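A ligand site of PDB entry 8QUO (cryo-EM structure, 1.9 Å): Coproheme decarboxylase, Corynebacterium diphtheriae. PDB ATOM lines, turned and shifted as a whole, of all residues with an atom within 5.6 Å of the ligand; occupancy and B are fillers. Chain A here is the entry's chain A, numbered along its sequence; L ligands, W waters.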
ATOM      1  N   ALA A 114     -15.004  -9.385  -0.779  1.00  0.00           N
ATOM      2  CA  ALA A 114     -16.252  -9.348  -1.526  1.00  0.00           C
ATOM      3  C   ALA A 114     -15.980  -9.179  -3.023  1.00  0.00           C
ATOM      4  O   ALA A 114     -14.920  -8.709  -3.440  1.00  0.00           O
ATOM      5  CB  ALA A 114     -17.144  -8.222  -1.016  1.00  0.00           C
ATOM      6  N   GLU A 115     -16.969  -9.578  -3.823  1.00  0.00           N
ATOM      7  CA  GLU A 115     -16.796  -9.573  -5.272  1.00  0.00           C
ATOM      8  C   GLU A 115     -16.731  -8.145  -5.813  1.00  0.00           C
ATOM      9  O   GLU A 115     -15.876  -7.833  -6.650  1.00  0.00           O
ATOM     10  CB  GLU A 115     -17.942 -10.340  -5.939  1.00  0.00           C
ATOM     11  CG  GLU A 115     -17.713 -10.623  -7.418  1.00  0.00           C
ATOM     12  CD  GLU A 115     -18.887 -11.338  -8.059  1.00  0.00           C
ATOM     13  OE1 GLU A 115     -19.978 -11.343  -7.453  1.00  0.00           O
ATOM     14  OE2 GLU A 115     -18.708 -11.895  -9.164  1.00  0.00           O
ATOM     15  N   PHE A 116     -17.626  -7.268  -5.354  1.00  0.00           N
ATOM     16  CA  PHE A 116     -17.738  -5.917  -5.906  1.00  0.00           C
ATOM     17  C   PHE A 116     -17.366  -4.844  -4.891  1.00  0.00           C
ATOM     18  O   PHE A 116     -16.475  -4.037  -5.146  1.00  0.00           O
ATOM     19  CB  PHE A 116     -19.154  -5.695  -6.440  1.00  0.00           C
ATOM     20  CG  PHE A 116     -19.560  -6.650  -7.531  1.00  0.00           C
ATOM     21  CD1 PHE A 116     -18.876  -6.667  -8.735  1.00  0.00           C
ATOM     22  CD2 PHE A 116     -20.602  -7.529  -7.338  1.00  0.00           C
ATOM     23  CE1 PHE A 116     -19.241  -7.546  -9.733  1.00  0.00           C
ATOM     24  CE2 PHE A 116     -20.974  -8.415  -8.339  1.00  0.00           C
ATOM     25  CZ  PHE A 116     -20.283  -8.425  -9.540  1.00  0.00           C
ATOM     26  N   ASN A 117     -18.031  -4.817  -3.734  1.00  0.00           N
ATOM     27  CA  ASN A 117     -17.779  -3.792  -2.727  1.00  0.00           C
ATOM     28  C   ASN A 117     -16.744  -4.329  -1.756  1.00  0.00           C
ATOM     29  O   ASN A 117     -17.071  -4.983  -0.758  1.00  0.00           O
ATOM     30  CB  ASN A 117     -19.073  -3.403  -2.025  1.00  0.00           C
ATOM     31  CG  ASN A 117     -18.874  -2.300  -0.994  1.00  0.00           C
ATOM     32  OD1 ASN A 117     -17.890  -1.568  -1.044  1.00  0.00           O
ATOM     33  ND2 ASN A 117     -19.805  -2.189  -0.063  1.00  0.00           N
ATOM     34  N   HIS A 120     -16.790  -3.732   2.175  1.00  0.00           N
ATOM     35  CA  HIS A 120     -17.654  -4.509   3.050  1.00  0.00           C
ATOM     36  C   HIS A 120     -16.876  -5.698   3.594  1.00  0.00           C
ATOM     37  O   HIS A 120     -16.437  -6.563   2.834  1.00  0.00           O
ATOM     38  CB  HIS A 120     -18.902  -4.978   2.300  1.00  0.00           C
ATOM     39  CG  HIS A 120     -19.922  -5.619   3.178  1.00  0.00           C
ATOM     40  ND1 HIS A 120     -20.292  -6.942   3.038  1.00  0.00           N
ATOM     41  CD2 HIS A 120     -20.666  -5.122   4.193  1.00  0.00           C
ATOM     42  CE1 HIS A 120     -21.214  -7.234   3.942  1.00  0.00           C
ATOM     43  NE2 HIS A 120     -21.466  -6.149   4.652  1.00  0.00           N
ATOM     44  N   TYR A 137     -27.109 -18.531   9.755  1.00  0.00           N
ATOM     45  CA  TYR A 137     -27.696 -19.497   8.835  1.00  0.00           C
ATOM     46  C   TYR A 137     -26.807 -19.651   7.616  1.00  0.00           C
ATOM     47  O   TYR A 137     -26.073 -18.722   7.259  1.00  0.00           O
ATOM     48  CB  TYR A 137     -29.119 -19.081   8.418  1.00  0.00           C
ATOM     49  CG  TYR A 137     -29.249 -17.715   7.785  1.00  0.00           C
ATOM     50  CD1 TYR A 137     -29.177 -16.558   8.548  1.00  0.00           C
ATOM     51  CD2 TYR A 137     -29.462 -17.581   6.418  1.00  0.00           C
ATOM     52  CE1 TYR A 137     -29.304 -15.320   7.981  1.00  0.00           C
ATOM     53  CE2 TYR A 137     -29.591 -16.339   5.843  1.00  0.00           C
ATOM     54  CZ  TYR A 137     -29.505 -15.214   6.619  1.00  0.00           C
ATOM     55  OH  TYR A 137     -29.625 -13.970   6.053  1.00  0.00           O
ATOM     56  N   PHE A 139     -26.349 -20.320   3.379  1.00  0.00           N
ATOM     57  CA  PHE A 139     -27.007 -19.734   2.218  1.00  0.00           C
ATOM     58  C   PHE A 139     -26.488 -20.407   0.955  1.00  0.00           C
ATOM     59  O   PHE A 139     -25.287 -20.636   0.814  1.00  0.00           O
ATOM     60  CB  PHE A 139     -26.746 -18.233   2.158  1.00  0.00           C
ATOM     61  CG  PHE A 139     -27.771 -17.478   1.362  1.00  0.00           C
ATOM     62  CD1 PHE A 139     -28.963 -17.095   1.926  1.00  0.00           C
ATOM     63  CD2 PHE A 139     -27.528 -17.154   0.036  1.00  0.00           C
ATOM     64  CE1 PHE A 139     -29.897 -16.396   1.192  1.00  0.00           C
ATOM     65  CE2 PHE A 139     -28.455 -16.461  -0.704  1.00  0.00           C
ATOM     66  CZ  PHE A 139     -29.649 -16.082  -0.118  1.00  0.00           C
ATOM     67  N   ARG A 141     -27.058 -19.878  -3.254  1.00  0.00           N
ATOM     68  CA  ARG A 141     -27.635 -19.054  -4.306  1.00  0.00           C
ATOM     69  C   ARG A 141     -28.237 -19.935  -5.399  1.00  0.00           C
ATOM     70  O   ARG A 141     -28.069 -21.148  -5.423  1.00  0.00           O
ATOM     71  CB  ARG A 141     -26.587 -18.115  -4.895  1.00  0.00           C
ATOM     72  CG  ARG A 141     -26.264 -16.913  -4.028  1.00  0.00           C
ATOM     73  CD  ARG A 141     -27.260 -15.799  -4.262  1.00  0.00           C
ATOM     74  NE  ARG A 141     -26.990 -14.639  -3.417  1.00  0.00           N
ATOM     75  CZ  ARG A 141     -27.921 -13.838  -2.924  1.00  0.00           C
ATOM     76  NH1 ARG A 141     -29.203 -14.029  -3.166  1.00  0.00           N
ATOM     77  NH2 ARG A 141     -27.554 -12.813  -2.162  1.00  0.00           N
ATOM     78  N   TRP A 145     -26.899 -17.789 -10.652  1.00  0.00           N
ATOM     79  CA  TRP A 145     -26.544 -16.540  -9.992  1.00  0.00           C
ATOM     80  C   TRP A 145     -25.144 -16.068 -10.378  1.00  0.00           C
ATOM     81  O   TRP A 145     -24.939 -14.878 -10.631  1.00  0.00           O
ATOM     82  CB  TRP A 145     -26.653 -16.708  -8.477  1.00  0.00           C
ATOM     83  CG  TRP A 145     -26.055 -15.593  -7.687  1.00  0.00           C
ATOM     84  CD1 TRP A 145     -24.874 -15.613  -7.007  1.00  0.00           C
ATOM     85  CD2 TRP A 145     -26.616 -14.296  -7.461  1.00  0.00           C
ATOM     86  NE1 TRP A 145     -24.661 -14.410  -6.386  1.00  0.00           N
ATOM     87  CE2 TRP A 145     -25.718 -13.579  -6.652  1.00  0.00           C
ATOM     88  CE3 TRP A 145     -27.795 -13.663  -7.872  1.00  0.00           C
ATOM     89  CZ2 TRP A 145     -25.958 -12.277  -6.245  1.00  0.00           C
ATOM     90  CZ3 TRP A 145     -28.029 -12.366  -7.470  1.00  0.00           C
ATOM     91  CH2 TRP A 145     -27.114 -11.682  -6.661  1.00  0.00           C
ATOM     92  N   TYR A 146     -24.182 -16.979 -10.432  1.00  0.00           N
ATOM     93  CA  TYR A 146     -22.804 -16.571 -10.636  1.00  0.00           C
ATOM     94  C   TYR A 146     -22.458 -16.340 -12.103  1.00  0.00           C
ATOM     95  O   TYR A 146     -21.553 -15.564 -12.405  1.00  0.00           O
ATOM     96  CB  TYR A 146     -21.851 -17.609 -10.024  1.00  0.00           C
ATOM     97  CG  TYR A 146     -22.080 -17.816  -8.548  1.00  0.00           C
ATOM     98  CD1 TYR A 146     -21.430 -17.028  -7.608  1.00  0.00           C
ATOM     99  CD2 TYR A 146     -22.949 -18.798  -8.092  1.00  0.00           C
ATOM    100  CE1 TYR A 146     -21.630 -17.212  -6.258  1.00  0.00           C
ATOM    101  CE2 TYR A 146     -23.157 -18.989  -6.744  1.00  0.00           C
ATOM    102  CZ  TYR A 146     -22.497 -18.202  -5.830  1.00  0.00           C
ATOM    103  OH  TYR A 146     -22.707 -18.388  -4.491  1.00  0.00           O
ATOM    104  N   ARG A 153     -25.683  -8.497 -11.692  1.00  0.00           N
ATOM    105  CA  ARG A 153     -25.482  -9.017 -10.336  1.00  0.00           C
ATOM    106  C   ARG A 153     -24.949  -7.922  -9.410  1.00  0.00           C
ATOM    107  O   ARG A 153     -25.347  -7.855  -8.240  1.00  0.00           O
ATOM    108  CB  ARG A 153     -24.527 -10.212 -10.367  1.00  0.00           C
ATOM    109  CG  ARG A 153     -24.336 -10.873  -9.009  1.00  0.00           C
ATOM    110  CD  ARG A 153     -23.561 -12.180  -9.118  1.00  0.00           C
ATOM    111  NE  ARG A 153     -22.228 -11.988  -9.665  1.00  0.00           N
ATOM    112  CZ  ARG A 153     -21.875 -12.299 -10.907  1.00  0.00           C
ATOM    113  NH1 ARG A 153     -22.739 -12.829 -11.758  1.00  0.00           N
ATOM    114  NH2 ARG A 153     -20.620 -12.087 -11.302  1.00  0.00           N
ATOM    115  N   LEU A 157     -26.815  -6.660  -6.060  1.00  0.00           N
ATOM    116  CA  LEU A 157     -26.158  -6.648  -4.760  1.00  0.00           C
ATOM    117  C   LEU A 157     -26.090  -5.253  -4.164  1.00  0.00           C
ATOM    118  O   LEU A 157     -26.182  -5.093  -2.948  1.00  0.00           O
ATOM    119  CB  LEU A 157     -24.758  -7.257  -4.880  1.00  0.00           C
ATOM    120  CG  LEU A 157     -24.711  -8.788  -4.955  1.00  0.00           C
ATOM    121  CD1 LEU A 157     -23.310  -9.272  -5.289  1.00  0.00           C
ATOM    122  CD2 LEU A 157     -25.189  -9.394  -3.651  1.00  0.00           C
ATOM    123  N   HIS A 160     -29.428  -4.631  -2.774  1.00  0.00           N
ATOM    124  CA  HIS A 160     -29.576  -5.461  -1.583  1.00  0.00           C
ATOM    125  C   HIS A 160     -28.898  -4.797  -0.390  1.00  0.00           C
ATOM    126  O   HIS A 160     -29.509  -4.620   0.675  1.00  0.00           O
ATOM    127  CB  HIS A 160     -28.996  -6.856  -1.895  1.00  0.00           C
ATOM    128  CG  HIS A 160     -28.448  -7.615  -0.713  1.00  0.00           C
ATOM    129  ND1 HIS A 160     -29.155  -8.646  -0.126  1.00  0.00           N
ATOM    130  CD2 HIS A 160     -27.267  -7.549  -0.067  1.00  0.00           C
ATOM    131  CE1 HIS A 160     -28.431  -9.169   0.852  1.00  0.00           C
ATOM    132  NE2 HIS A 160     -27.280  -8.515   0.913  1.00  0.00           N
ATOM    133  N   GLY A 161     -27.668  -4.323  -0.586  1.00  0.00           N
ATOM    134  CA  GLY A 161     -26.955  -3.625   0.475  1.00  0.00           C
ATOM    135  C   GLY A 161     -27.617  -2.320   0.875  1.00  0.00           C
ATOM    136  O   GLY A 161     -27.646  -1.963   2.061  1.00  0.00           O
ATOM    137  N   ALA A 164     -30.497  -2.370   3.474  1.00  0.00           N
ATOM    138  CA  ALA A 164     -30.165  -2.524   4.881  1.00  0.00           C
ATOM    139  C   ALA A 164     -29.585  -1.244   5.488  1.00  0.00           C
ATOM    140  O   ALA A 164     -28.923  -1.308   6.540  1.00  0.00           O
ATOM    141  CB  ALA A 164     -29.194  -3.689   5.079  1.00  0.00           C
ATOM    142  N   PHE A 167     -30.535  -0.172   9.248  1.00  0.00           N
ATOM    143  CA  PHE A 167     -30.145  -1.027  10.366  1.00  0.00           C
ATOM    144  C   PHE A 167     -28.630  -0.993  10.513  1.00  0.00           C
ATOM    145  O   PHE A 167     -27.948  -2.003  10.294  1.00  0.00           O
ATOM    146  CB  PHE A 167     -30.635  -2.455  10.160  1.00  0.00           C
ATOM    147  CG  PHE A 167     -32.131  -2.573  10.030  1.00  0.00           C
ATOM    148  CD1 PHE A 167     -32.752  -2.395   8.809  1.00  0.00           C
ATOM    149  CD2 PHE A 167     -32.910  -2.858  11.139  1.00  0.00           C
ATOM    150  CE1 PHE A 167     -34.122  -2.504   8.699  1.00  0.00           C
ATOM    151  CE2 PHE A 167     -34.280  -2.967  11.028  1.00  0.00           C
ATOM    152  CZ  PHE A 167     -34.887  -2.788   9.804  1.00  0.00           C
ATOM    153  N   VAL A 170     -27.029  -3.437  13.267  1.00  0.00           N
ATOM    154  CA  VAL A 170     -26.937  -4.866  13.003  1.00  0.00           C
ATOM    155  C   VAL A 170     -25.706  -5.093  12.139  1.00  0.00           C
ATOM    156  O   VAL A 170     -25.646  -4.647  10.993  1.00  0.00           O
ATOM    157  CB  VAL A 170     -28.207  -5.409  12.323  1.00  0.00           C
ATOM    158  CG1 VAL A 170     -28.084  -6.902  12.108  1.00  0.00           C
ATOM    159  CG2 VAL A 170     -29.433  -5.074  13.154  1.00  0.00           C
ATOM    160  N   ARG A 171     -24.723  -5.800  12.689  1.00  0.00           N
ATOM    161  CA  ARG A 171     -23.474  -6.071  11.998  1.00  0.00           C
ATOM    162  C   ARG A 171     -23.572  -7.408  11.278  1.00  0.00           C
ATOM    163  O   ARG A 171     -24.046  -8.399  11.851  1.00  0.00           O
ATOM    164  CB  ARG A 171     -22.296  -6.075  12.973  1.00  0.00           C
ATOM    165  CG  ARG A 171     -22.286  -4.898  13.931  1.00  0.00           C
ATOM    166  CD  ARG A 171     -22.361  -3.574  13.199  1.00  0.00           C
ATOM    167  NE  ARG A 171     -21.258  -3.406  12.270  1.00  0.00           N
ATOM    168  CZ  ARG A 171     -21.259  -2.561  11.245  1.00  0.00           C
ATOM    169  NH1 ARG A 171     -22.295  -1.785  10.988  1.00  0.00           N
ATOM    170  NH2 ARG A 171     -20.183  -2.484  10.460  1.00  0.00           N
ATOM    171  N   ALA A 172     -23.123  -7.430  10.026  1.00  0.00           N
ATOM    172  CA  ALA A 172     -23.263  -8.585   9.151  1.00  0.00           C
ATOM    173  C   ALA A 172     -21.915  -9.249   8.903  1.00  0.00           C
ATOM    174  O   ALA A 172     -20.897  -8.566   8.754  1.00  0.00           O
ATOM    175  CB  ALA A 172     -23.898  -8.178   7.819  1.00  0.00           C
ATOM    176  N   THR A 174     -20.668 -12.082   6.191  1.00  0.00           N
ATOM    177  CA  THR A 174     -20.975 -12.892   5.015  1.00  0.00           C
ATOM    178  C   THR A 174     -19.687 -13.543   4.553  1.00  0.00           C
ATOM    179  O   THR A 174     -18.803 -12.863   4.009  1.00  0.00           O
ATOM    180  CB  THR A 174     -21.583 -12.030   3.899  1.00  0.00           C
ATOM    181  OG1 THR A 174     -22.857 -11.519   4.334  1.00  0.00           O
ATOM    182  CG2 THR A 174     -21.761 -12.845   2.639  1.00  0.00           C
ATOM    183  N   TRP A 185     -22.483 -20.019   1.302  1.00  0.00           N
ATOM    184  CA  TRP A 185     -22.149 -18.897   2.153  1.00  0.00           C
ATOM    185  C   TRP A 185     -22.617 -19.162   3.574  1.00  0.00           C
ATOM    186  O   TRP A 185     -23.543 -19.940   3.809  1.00  0.00           O
ATOM    187  CB  TRP A 185     -22.785 -17.586   1.644  1.00  0.00           C
ATOM    188  CG  TRP A 185     -22.368 -17.207   0.269  1.00  0.00           C
ATOM    189  CD1 TRP A 185     -22.949 -17.609  -0.901  1.00  0.00           C
ATOM    190  CD2 TRP A 185     -21.288 -16.342  -0.097  1.00  0.00           C
ATOM    191  NE1 TRP A 185     -22.294 -17.055  -1.972  1.00  0.00           N
ATOM    192  CE2 TRP A 185     -21.264 -16.268  -1.502  1.00  0.00           C
ATOM    193  CE3 TRP A 185     -20.345 -15.616   0.623  1.00  0.00           C
ATOM    194  CZ2 TRP A 185     -20.339 -15.507  -2.199  1.00  0.00           C
ATOM    195  CZ3 TRP A 185     -19.418 -14.860  -0.066  1.00  0.00           C
ATOM    196  CH2 TRP A 185     -19.420 -14.805  -1.464  1.00  0.00           C
ATOM    197  N   LEU A 187     -23.831 -16.856   6.907  1.00  0.00           N
ATOM    198  CA  LEU A 187     -24.274 -15.515   7.259  1.00  0.00           C
ATOM    199  C   LEU A 187     -24.539 -15.451   8.749  1.00  0.00           C
ATOM    200  O   LEU A 187     -25.214 -16.329   9.311  1.00  0.00           O
ATOM    201  CB  LEU A 187     -25.524 -15.137   6.476  1.00  0.00           C
ATOM    202  CG  LEU A 187     -25.495 -15.424   4.975  1.00  0.00           C
ATOM    203  CD1 LEU A 187     -26.777 -14.989   4.306  1.00  0.00           C
ATOM    204  CD2 LEU A 187     -24.306 -14.737   4.331  1.00  0.00           C
ATOM    205  N   PHE A 189     -25.567 -12.443  11.782  1.00  0.00           N
ATOM    206  CA  PHE A 189     -25.964 -11.077  12.089  1.00  0.00           C
ATOM    207  C   PHE A 189     -25.982 -10.893  13.598  1.00  0.00           C
ATOM    208  O   PHE A 189     -26.627 -11.658  14.315  1.00  0.00           O
ATOM    209  CB  PHE A 189     -27.338 -10.757  11.484  1.00  0.00           C
ATOM    210  CG  PHE A 189     -27.371 -10.893   9.993  1.00  0.00           C
ATOM    211  CD1 PHE A 189     -26.996  -9.830   9.190  1.00  0.00           C
ATOM    212  CD2 PHE A 189     -27.753 -12.076   9.404  1.00  0.00           C
ATOM    213  CE1 PHE A 189     -27.021  -9.951   7.813  1.00  0.00           C
ATOM    214  CE2 PHE A 189     -27.779 -12.196   8.027  1.00  0.00           C
ATOM    215  CZ  PHE A 189     -27.408 -11.133   7.237  1.00  0.00           C
ATOM    216  N   LEU A 200     -34.818  -6.422  10.467  1.00  0.00           N
ATOM    217  CA  LEU A 200     -33.915  -6.419   9.314  1.00  0.00           C
ATOM    218  C   LEU A 200     -34.221  -7.572   8.375  1.00  0.00           C
ATOM    219  O   LEU A 200     -34.238  -7.407   7.155  1.00  0.00           O
ATOM    220  CB  LEU A 200     -32.465  -6.473   9.770  1.00  0.00           C
ATOM    221  CG  LEU A 200     -31.458  -6.754   8.648  1.00  0.00           C
ATOM    222  CD1 LEU A 200     -31.145  -5.486   7.876  1.00  0.00           C
ATOM    223  CD2 LEU A 200     -30.192  -7.374   9.199  1.00  0.00           C
ATOM    224  N   MET A 201     -34.455  -8.766   8.932  1.00  0.00           N
ATOM    225  CA  MET A 201     -34.783  -9.915   8.099  1.00  0.00           C
ATOM    226  C   MET A 201     -36.095  -9.709   7.361  1.00  0.00           C
ATOM    227  O   MET A 201     -36.222 -10.082   6.184  1.00  0.00           O
ATOM    228  CB  MET A 201     -34.831 -11.190   8.952  1.00  0.00           C
ATOM    229  CG  MET A 201     -34.472 -12.465   8.196  1.00  0.00           C
ATOM    230  SD  MET A 201     -32.730 -12.610   7.724  1.00  0.00           S
ATOM    231  CE  MET A 201     -31.905 -11.763   9.071  1.00  0.00           C
ATOM    232  N   MET A 204     -35.431  -7.135   4.530  1.00  0.00           N
ATOM    233  CA  MET A 204     -34.577  -7.626   3.454  1.00  0.00           C
ATOM    234  C   MET A 204     -35.316  -8.514   2.466  1.00  0.00           C
ATOM    235  O   MET A 204     -34.755  -8.835   1.412  1.00  0.00           O
ATOM    236  CB  MET A 204     -33.379  -8.378   4.040  1.00  0.00           C
ATOM    237  CG  MET A 204     -32.310  -7.469   4.608  1.00  0.00           C
ATOM    238  SD  MET A 204     -31.750  -6.221   3.449  1.00  0.00           S
ATOM    239  CE  MET A 204     -30.342  -7.065   2.721  1.00  0.00           C
ATOM    240  N   ARG A 205     -36.547  -8.933   2.779  1.00  0.00           N
ATOM    241  CA  ARG A 205     -37.339  -9.701   1.828  1.00  0.00           C
ATOM    242  C   ARG A 205     -37.768  -8.856   0.630  1.00  0.00           C
ATOM    243  O   ARG A 205     -38.164  -9.425  -0.391  1.00  0.00           O
ATOM    244  CB  ARG A 205     -38.573 -10.280   2.512  1.00  0.00           C
ATOM    245  CG  ARG A 205     -38.270 -11.412   3.477  1.00  0.00           C
ATOM    246  CD  ARG A 205     -37.629 -12.579   2.759  1.00  0.00           C
ATOM    247  NE  ARG A 205     -37.855 -13.843   3.463  1.00  0.00           N
ATOM    248  CZ  ARG A 205     -36.976 -14.415   4.264  1.00  0.00           C
ATOM    249  NH1 ARG A 205     -35.803 -13.861   4.523  1.00  0.00           N
ATOM    250  NH2 ARG A 205     -37.287 -15.580   4.846  1.00  0.00           N
ATOM    251  N   ARG A 210     -33.828 -11.767  -3.552  1.00  0.00           N
ATOM    252  CA  ARG A 210     -34.666 -12.869  -3.103  1.00  0.00           C
ATOM    253  C   ARG A 210     -35.097 -13.778  -4.257  1.00  0.00           C
ATOM    254  O   ARG A 210     -35.502 -14.919  -4.005  1.00  0.00           O
ATOM    255  CB  ARG A 210     -35.903 -12.339  -2.380  1.00  0.00           C
ATOM    256  CG  ARG A 210     -35.592 -11.546  -1.121  1.00  0.00           C
ATOM    257  CD  ARG A 210     -34.893 -12.416  -0.093  1.00  0.00           C
ATOM    258  NE  ARG A 210     -35.668 -13.607   0.239  1.00  0.00           N
ATOM    259  CZ  ARG A 210     -35.205 -14.631   0.940  1.00  0.00           C
ATOM    260  NH1 ARG A 210     -33.967 -14.656   1.399  1.00  0.00           N
ATOM    261  NH2 ARG A 210     -36.006 -15.663   1.182  1.00  0.00           N
ATOM    262  N   GLU A 216     -31.683 -21.414   2.593  1.00  0.00           N
ATOM    263  CA  GLU A 216     -31.284 -20.482   3.638  1.00  0.00           C
ATOM    264  C   GLU A 216     -31.605 -21.013   5.029  1.00  0.00           C
ATOM    265  O   GLU A 216     -31.804 -20.232   5.962  1.00  0.00           O
ATOM    266  CB  GLU A 216     -31.935 -19.115   3.428  1.00  0.00           C
ATOM    267  CG  GLU A 216     -33.447 -19.161   3.357  1.00  0.00           C
ATOM    268  CD  GLU A 216     -34.042 -17.841   2.914  1.00  0.00           C
ATOM    269  OE1 GLU A 216     -33.532 -16.785   3.335  1.00  0.00           O
ATOM    270  OE2 GLU A 216     -35.030 -17.860   2.137  1.00  0.00           O
HETATM  271  C1  LIG L   1     -23.153  -9.854   0.142  1.00  0.00           C
HETATM  272  C2  LIG L   1     -24.735  -5.996   2.621  1.00  0.00           C
HETATM  273  C3  LIG L   1     -28.019  -8.764   4.846  1.00  0.00           C
HETATM  274  C4  LIG L   1     -26.913 -12.401   1.849  1.00  0.00           C
HETATM  275  C5  LIG L   1     -23.271  -8.564   0.605  1.00  0.00           C
HETATM  276  C6  LIG L   1     -22.472  -7.414   0.231  1.00  0.00           C
HETATM  277  C7  LIG L   1     -22.915  -6.357   0.915  1.00  0.00           C
HETATM  278  C8  LIG L   1     -24.012  -6.787   1.759  1.00  0.00           C
HETATM  279  C9  LIG L   1     -22.365  -4.915   0.828  1.00  0.00           C
HETATM  280  C10 LIG L   1     -21.305  -7.362  -0.783  1.00  0.00           C
HETATM  281  C11 LIG L   1     -21.753  -7.806  -2.169  1.00  0.00           C
HETATM  282  C12 LIG L   1     -20.680  -7.453  -3.160  1.00  0.00           C
HETATM  283  O1  LIG L   1     -20.047  -8.382  -3.711  1.00  0.00           O
HETATM  284  O2  LIG L   1     -20.466  -6.237  -3.389  1.00  0.00           O
HETATM  285  C13 LIG L   1     -25.626  -6.468   3.565  1.00  0.00           C
HETATM  286  C14 LIG L   1     -25.938  -5.849   4.825  1.00  0.00           C
HETATM  287  C15 LIG L   1     -26.856  -6.609   5.450  1.00  0.00           C
HETATM  288  C16 LIG L   1     -27.143  -7.744   4.577  1.00  0.00           C
HETATM  289  C17 LIG L   1     -25.286  -4.530   5.305  1.00  0.00           C
HETATM  290  C18 LIG L   1     -27.546  -6.434   6.832  1.00  0.00           C
HETATM  291  C19 LIG L   1     -27.312  -5.428   7.677  1.00  0.00           C
HETATM  292  C20 LIG L   1     -28.101  -9.942   4.133  1.00  0.00           C
HETATM  293  C21 LIG L   1     -29.192 -10.897   4.163  1.00  0.00           C
HETATM  294  C22 LIG L   1     -28.885 -11.915   3.335  1.00  0.00           C
HETATM  295  C23 LIG L   1     -27.590 -11.614   2.756  1.00  0.00           C
HETATM  296  C24 LIG L   1     -30.454 -10.702   5.039  1.00  0.00           C
HETATM  297  C25 LIG L   1     -29.681 -13.194   2.976  1.00  0.00           C
HETATM  298  C26 LIG L   1     -30.931 -13.457   3.375  1.00  0.00           C
HETATM  299  C27 LIG L   1     -25.744 -12.065   1.204  1.00  0.00           C
HETATM  300  C28 LIG L   1     -24.900 -12.975   0.454  1.00  0.00           C
HETATM  301  C29 LIG L   1     -23.866 -12.280  -0.025  1.00  0.00           C
HETATM  302  C30 LIG L   1     -24.005 -10.901   0.413  1.00  0.00           C
HETATM  303  C31 LIG L   1     -25.161 -14.479   0.239  1.00  0.00           C
HETATM  304  C32 LIG L   1     -22.722 -12.881  -0.873  1.00  0.00           C
HETATM  305  C33 LIG L   1     -22.648 -12.229  -2.246  1.00  0.00           C
HETATM  306  C34 LIG L   1     -23.318 -13.123  -3.256  1.00  0.00           C
HETATM  307  O3  LIG L   1     -22.868 -13.139  -4.433  1.00  0.00           O
HETATM  308  O4  LIG L   1     -24.280 -13.830  -2.887  1.00  0.00           O
HETATM  309  N1  LIG L   1     -24.200  -8.144   1.540  1.00  0.00           N
HETATM  310  N2  LIG L   1     -26.369  -7.625   3.443  1.00  0.00           N
HETATM  311  N3  LIG L   1     -27.141 -10.413   3.255  1.00  0.00           N
HETATM  312  N4  LIG L   1     -25.169 -10.810   1.154  1.00  0.00           N
HETATM  313 FE1  LIG L   1     -25.753  -9.232   2.316  1.00  0.00          FE
HETATM  314  O   HOH W   1     -19.664 -10.646  -2.496  1.00  0.00           O
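The backbone NH (N) of Phe 139 is in hydrogen-bond range of the backbone carbonyl oxygen (O) of Trp 185.
OE2 of Glu 216 lies within salt-bridge range of NH2 of Arg 210.
N of Leu 187 sits at hydrogen-bond distance from O of Tyr 137 (2.9 Å).
O of Trp 145 sits at hydrogen-bond distance from NH1 of Arg 153 (3.2 Å).
NE1 of Trp 185 lies within hydrogen-bond range of OH of Tyr 146 (2.9 Å).
NH2 of Arg 153 lies within salt-bridge range of OE2 of Glu 115 (2.9 Å).
OH of Tyr 137 sits at hydrogen-bond distance from SD of Met 201 (3.8 Å).
Water W1 lies within hydrogen-bond range of O1 of the ligand (2.6 Å) and N of Glu 115 (3.2 Å).
Merely in contact with the ligand: Tyr 137 (3.0 Å), Phe 189 (3.3 Å), His 120 (3.4 Å), Thr 174 (3.4 Å), Leu 187 (3.6 Å), Met 204 (3.6 Å), Phe 139 (3.6 Å), Ala 164 (3.6 Å), Leu 200 (3.7 Å), Leu 157 (3.7 Å), Trp 185 (3.7 Å), Val 170 (3.8 Å), Arg 210 (3.8 Å), Gly 161 (3.9 Å) and Ala 114 (3.96 Å).
Hydrophobic or aromatic side chains that line the ligand: Ala 114, Phe 116, His 120, Tyr 137, Phe 139, Trp 145, Leu 157, His 160, Ala 164, Trp 185, Leu 187, Phe 189, Leu 200 and Met 204.
21 residues have an atom within 4 Å of the ligand: Ala 114, Glu 115, Phe 116, Asn 117, His 120, Tyr 137, Phe 139, Arg 141, Trp 145, Leu 157, His 160, Gly 161, Ala 164, Val 170, Thr 174, Trp 185, Leu 187, Phe 189, Leu 200, Met 204 and Arg 210.
The indole nitrogen (NE1) of Trp 145 sits at hydrogen-bond distance from an oxygen (O3) of the ligand.
O1 of the ligand is in hydrogen-bond range of N of Glu 115 (3.3 Å).
N of Asn 117 lies within hydrogen-bond range of O2 of the ligand (2.8 Å).
The backbone NH (N) of Phe 116 lies within hydrogen-bond range of an oxygen (O1) of the ligand.
O4 of the ligand lies within salt-bridge range of NE of Arg 141, 2.9 Å away.
NE2 of His 160 is bound to FE1 of the ligand (2.2 Å).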
